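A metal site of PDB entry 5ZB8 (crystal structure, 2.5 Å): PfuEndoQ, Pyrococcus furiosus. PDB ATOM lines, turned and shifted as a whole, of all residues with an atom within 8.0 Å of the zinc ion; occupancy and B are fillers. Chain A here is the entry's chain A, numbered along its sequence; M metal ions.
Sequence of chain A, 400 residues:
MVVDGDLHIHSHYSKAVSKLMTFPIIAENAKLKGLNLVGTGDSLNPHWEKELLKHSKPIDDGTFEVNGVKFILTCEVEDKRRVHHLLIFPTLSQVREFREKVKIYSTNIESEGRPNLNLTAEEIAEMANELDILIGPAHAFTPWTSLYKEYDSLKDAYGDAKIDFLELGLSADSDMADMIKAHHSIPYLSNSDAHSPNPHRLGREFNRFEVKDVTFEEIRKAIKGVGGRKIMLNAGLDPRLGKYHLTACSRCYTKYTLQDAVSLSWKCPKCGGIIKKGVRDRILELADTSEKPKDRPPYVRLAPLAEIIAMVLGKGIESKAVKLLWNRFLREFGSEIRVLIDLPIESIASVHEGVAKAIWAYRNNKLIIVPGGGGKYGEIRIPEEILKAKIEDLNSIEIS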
ATOM      1  N   ALA A 248       9.183  33.625   4.551  1.00  0.00           N
ATOM      2  CA  ALA A 248       8.913  32.806   5.722  1.00  0.00           C
ATOM      3  C   ALA A 248       9.196  31.347   5.405  1.00  0.00           C
ATOM      4  O   ALA A 248       9.155  30.916   4.256  1.00  0.00           O
ATOM      5  CB  ALA A 248       7.458  32.966   6.186  1.00  0.00           C
ATOM      6  N   CYS A 249       9.499  30.586   6.464  1.00  0.00           N
ATOM      7  CA  CYS A 249       9.655  29.142   6.319  1.00  0.00           C
ATOM      8  C   CYS A 249       8.326  28.509   5.931  1.00  0.00           C
ATOM      9  O   CYS A 249       7.268  28.852   6.456  1.00  0.00           O
ATOM     10  CB  CYS A 249      10.171  28.538   7.626  1.00  0.00           C
ATOM     11  SG  CYS A 249      10.201  26.728   7.643  1.00  0.00           S
ATOM     12  N   SER A 250       8.383  27.573   4.987  1.00  0.00           N
ATOM     13  CA  SER A 250       7.174  26.928   4.488  1.00  0.00           C
ATOM     14  C   SER A 250       6.662  25.831   5.407  1.00  0.00           C
ATOM     15  O   SER A 250       5.631  25.221   5.102  1.00  0.00           O
ATOM     16  CB  SER A 250       7.422  26.350   3.086  1.00  0.00           C
ATOM     17  OG  SER A 250       8.457  25.392   3.102  1.00  0.00           O
ATOM     18  N   ARG A 251       7.332  25.573   6.530  1.00  0.00           N
ATOM     19  CA  ARG A 251       6.923  24.548   7.477  1.00  0.00           C
ATOM     20  C   ARG A 251       6.457  25.123   8.808  1.00  0.00           C
ATOM     21  O   ARG A 251       5.375  24.764   9.284  1.00  0.00           O
ATOM     22  CB  ARG A 251       8.056  23.545   7.707  1.00  0.00           C
ATOM     23  CG  ARG A 251       7.736  22.493   8.758  1.00  0.00           C
ATOM     24  CD  ARG A 251       8.260  21.132   8.337  1.00  0.00           C
ATOM     25  NE  ARG A 251       9.711  21.036   8.403  1.00  0.00           N
ATOM     26  CZ  ARG A 251      10.421  20.157   7.692  1.00  0.00           C
ATOM     27  NH1 ARG A 251       9.817  19.324   6.874  1.00  0.00           N
ATOM     28  NH2 ARG A 251      11.747  20.133   7.808  1.00  0.00           N
ATOM     29  N   CYS A 252       7.245  26.002   9.428  1.00  0.00           N
ATOM     30  CA  CYS A 252       6.865  26.596  10.700  1.00  0.00           C
ATOM     31  C   CYS A 252       6.413  28.042  10.570  1.00  0.00           C
ATOM     32  O   CYS A 252       5.959  28.619  11.568  1.00  0.00           O
ATOM     33  CB  CYS A 252       8.037  26.525  11.694  1.00  0.00           C
ATOM     34  SG  CYS A 252       9.365  27.718  11.374  1.00  0.00           S
ATOM     35  N   TYR A 253       6.531  28.640   9.388  1.00  0.00           N
ATOM     36  CA  TYR A 253       5.991  29.961   9.058  1.00  0.00           C
ATOM     37  C   TYR A 253       6.644  31.084   9.854  1.00  0.00           C
ATOM     38  O   TYR A 253       6.099  32.195   9.922  1.00  0.00           O
ATOM     39  CB  TYR A 253       4.471  29.993   9.241  1.00  0.00           C
ATOM     40  CG  TYR A 253       3.797  28.843   8.538  1.00  0.00           C
ATOM     41  CD1 TYR A 253       3.745  28.795   7.148  1.00  0.00           C
ATOM     42  CD2 TYR A 253       3.226  27.801   9.249  1.00  0.00           C
ATOM     43  CE1 TYR A 253       3.135  27.746   6.497  1.00  0.00           C
ATOM     44  CE2 TYR A 253       2.617  26.742   8.608  1.00  0.00           C
ATOM     45  CZ  TYR A 253       2.566  26.715   7.228  1.00  0.00           C
ATOM     46  OH  TYR A 253       1.966  25.675   6.576  1.00  0.00           O
ATOM     47  N   THR A 254       7.810  30.832  10.441  1.00  0.00           N
ATOM     48  CA  THR A 254       8.586  31.910  11.047  1.00  0.00           C
ATOM     49  C   THR A 254       9.054  32.882   9.965  1.00  0.00           C
ATOM     50  O   THR A 254       9.555  32.464   8.918  1.00  0.00           O
ATOM     51  CB  THR A 254       9.795  31.332  11.790  1.00  0.00           C
ATOM     52  OG1 THR A 254       9.357  30.367  12.749  1.00  0.00           O
ATOM     53  CG2 THR A 254      10.562  32.443  12.506  1.00  0.00           C
ATOM     54  N   LYS A 255       8.877  34.179  10.216  1.00  0.00           N
ATOM     55  CA  LYS A 255       9.244  35.183   9.243  1.00  0.00           C
ATOM     56  C   LYS A 255      10.728  35.508   9.335  1.00  0.00           C
ATOM     57  O   LYS A 255      11.295  35.579  10.428  1.00  0.00           O
ATOM     58  CB  LYS A 255       8.419  36.458   9.441  1.00  0.00           C
ATOM     59  CG  LYS A 255       6.940  36.224   9.748  1.00  0.00           C
ATOM     60  CD  LYS A 255       6.243  35.413   8.676  1.00  0.00           C
ATOM     61  CE  LYS A 255       4.811  35.101   9.061  1.00  0.00           C
ATOM     62  NZ  LYS A 255       4.226  33.997   8.239  1.00  0.00           N
ATOM     63  N   TYR A 256      11.349  35.708   8.180  1.00  0.00           N
ATOM     64  CA  TYR A 256      12.758  36.088   8.097  1.00  0.00           C
ATOM     65  C   TYR A 256      12.905  37.252   7.128  1.00  0.00           C
ATOM     66  O   TYR A 256      12.166  37.365   6.145  1.00  0.00           O
ATOM     67  CB  TYR A 256      13.639  34.926   7.629  1.00  0.00           C
ATOM     68  CG  TYR A 256      13.637  33.710   8.526  1.00  0.00           C
ATOM     69  CD1 TYR A 256      14.570  33.580   9.553  1.00  0.00           C
ATOM     70  CD2 TYR A 256      12.707  32.693   8.345  1.00  0.00           C
ATOM     71  CE1 TYR A 256      14.571  32.462  10.377  1.00  0.00           C
ATOM     72  CE2 TYR A 256      12.707  31.575   9.158  1.00  0.00           C
ATOM     73  CZ  TYR A 256      13.639  31.464  10.174  1.00  0.00           C
ATOM     74  OH  TYR A 256      13.628  30.356  10.979  1.00  0.00           O
ATOM     75  N   LYS A 267      17.466  27.799   4.275  1.00  0.00           N
ATOM     76  CA  LYS A 267      17.129  26.765   5.257  1.00  0.00           C
ATOM     77  C   LYS A 267      16.743  27.430   6.568  1.00  0.00           C
ATOM     78  O   LYS A 267      17.493  28.256   7.102  1.00  0.00           O
ATOM     79  CB  LYS A 267      18.291  25.802   5.462  1.00  0.00           C
ATOM     80  CG  LYS A 267      18.035  24.771   6.557  1.00  0.00           C
ATOM     81  CD  LYS A 267      19.251  23.899   6.816  1.00  0.00           C
ATOM     82  CE  LYS A 267      19.033  22.971   7.995  1.00  0.00           C
ATOM     83  NZ  LYS A 267      18.844  23.725   9.266  1.00  0.00           N
ATOM     84  N   CYS A 268      15.584  27.062   7.091  1.00  0.00           N
ATOM     85  CA  CYS A 268      15.124  27.606   8.362  1.00  0.00           C
ATOM     86  C   CYS A 268      15.926  26.988   9.503  1.00  0.00           C
ATOM     87  O   CYS A 268      15.985  25.761   9.612  1.00  0.00           O
ATOM     88  CB  CYS A 268      13.634  27.349   8.550  1.00  0.00           C
ATOM     89  SG  CYS A 268      13.005  27.742  10.191  1.00  0.00           S
ATOM     90  N   PRO A 269      16.545  27.793  10.371  1.00  0.00           N
ATOM     91  CA  PRO A 269      17.296  27.225  11.506  1.00  0.00           C
ATOM     92  C   PRO A 269      16.411  26.744  12.641  1.00  0.00           C
ATOM     93  O   PRO A 269      16.924  26.100  13.568  1.00  0.00           O
ATOM     94  CB  PRO A 269      18.179  28.389  11.949  1.00  0.00           C
ATOM     95  CG  PRO A 269      17.378  29.599  11.615  1.00  0.00           C
ATOM     96  CD  PRO A 269      16.624  29.263  10.344  1.00  0.00           C
ATOM     97  N   LYS A 270      15.115  27.041  12.616  1.00  0.00           N
ATOM     98  CA  LYS A 270      14.215  26.649  13.700  1.00  0.00           C
ATOM     99  C   LYS A 270      13.739  25.213  13.540  1.00  0.00           C
ATOM    100  O   LYS A 270      13.742  24.439  14.504  1.00  0.00           O
ATOM    101  CB  LYS A 270      13.037  27.619  13.766  1.00  0.00           C
ATOM    102  CG  LYS A 270      12.007  27.307  14.839  1.00  0.00           C
ATOM    103  CD  LYS A 270      10.892  28.335  14.819  1.00  0.00           C
ATOM    104  CE  LYS A 270       9.907  28.124  15.955  1.00  0.00           C
ATOM    105  NZ  LYS A 270       8.843  29.162  15.950  1.00  0.00           N
ATOM    106  N   CYS A 271      13.331  24.840  12.330  1.00  0.00           N
ATOM    107  CA  CYS A 271      12.816  23.502  12.081  1.00  0.00           C
ATOM    108  C   CYS A 271      13.476  22.801  10.907  1.00  0.00           C
ATOM    109  O   CYS A 271      13.128  21.642  10.618  1.00  0.00           O
ATOM    110  CB  CYS A 271      11.299  23.542  11.831  1.00  0.00           C
ATOM    111  SG  CYS A 271      10.828  24.249  10.236  1.00  0.00           S
ATOM    112  N   GLY A 272      14.419  23.444  10.214  1.00  0.00           N
ATOM    113  CA  GLY A 272      15.052  22.833   9.071  1.00  0.00           C
ATOM    114  C   GLY A 272      14.266  22.917   7.782  1.00  0.00           C
ATOM    115  O   GLY A 272      14.641  22.271   6.803  1.00  0.00           O
ATOM    116  N   GLY A 273      13.180  23.685   7.756  1.00  0.00           N
ATOM    117  CA  GLY A 273      12.344  23.771   6.571  1.00  0.00           C
ATOM    118  C   GLY A 273      12.885  24.714   5.524  1.00  0.00           C
ATOM    119  O   GLY A 273      13.856  25.441   5.720  1.00  0.00           O
ATOM    120  N   ILE A 274      12.211  24.702   4.368  1.00  0.00           N
ATOM    121  CA  ILE A 274      12.614  25.522   3.226  1.00  0.00           C
ATOM    122  C   ILE A 274      11.954  26.895   3.357  1.00  0.00           C
ATOM    123  O   ILE A 274      10.717  26.995   3.443  1.00  0.00           O
ATOM    124  CB  ILE A 274      12.226  24.855   1.903  1.00  0.00           C
ATOM    125  CG1 ILE A 274      12.879  23.473   1.803  1.00  0.00           C
ATOM    126  CG2 ILE A 274      12.636  25.724   0.728  1.00  0.00           C
ATOM    127  CD1 ILE A 274      12.441  22.679   0.588  1.00  0.00           C
ATOM    128  N   ILE A 275      12.760  27.947   3.378  1.00  0.00           N
ATOM    129  CA  ILE A 275      12.244  29.308   3.436  1.00  0.00           C
ATOM    130  C   ILE A 275      11.801  29.730   2.048  1.00  0.00           C
ATOM    131  O   ILE A 275      12.507  29.514   1.058  1.00  0.00           O
ATOM    132  CB  ILE A 275      13.307  30.265   3.990  1.00  0.00           C
ATOM    133  CG1 ILE A 275      13.827  29.773   5.344  1.00  0.00           C
ATOM    134  CG2 ILE A 275      12.748  31.659   4.131  1.00  0.00           C
ATOM    135  CD1 ILE A 275      14.903  30.651   5.938  1.00  0.00           C
HETATM  136 ZN    ZN M   1      10.834  26.582   9.941  1.00  0.00          ZN
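SG of Cys 252 lies close to OG1 of Thr 254 (3.0 Å). The side-chain sulfur (SG) of Cys 271 lies close to the backbone NH (N) of Gly 273 (3.5 Å). The backbone carbonyl oxygen of Cys 271 lies within hydrogen-bond range of the guanidinium group of Arg 251, at 3.5 Å. SG of Cys 249 sits close to N of Arg 251 (3.3 Å). N of Cys 249 sits at hydrogen-bond distance from O of Thr 254. The backbone carbonyl oxygen (O) of Gly 273 sits at hydrogen-bond distance from the backbone NH (N) of Cys 268. The side-chain sulfur of Cys 268 lies close to the backbone NH of Lys 270, at 3.3 Å. SG of Cys 268 lies close to OH of Tyr 256, at 2.8 Å.
Within 4 Å of the zinc ion: Cys 249, Cys 252, Cys 268 and Cys 271.
The zinc ion is bound by SG of Cys 252 (2.3 Å). The zinc ion is bound by the side-chain sulfur (SG) of Cys 271. The zinc ion is bound by the side-chain sulfur (SG) of Cys 249 (2.4 Å). SG of Cys 268 is bound to the zinc ion, 2.5 Å away.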
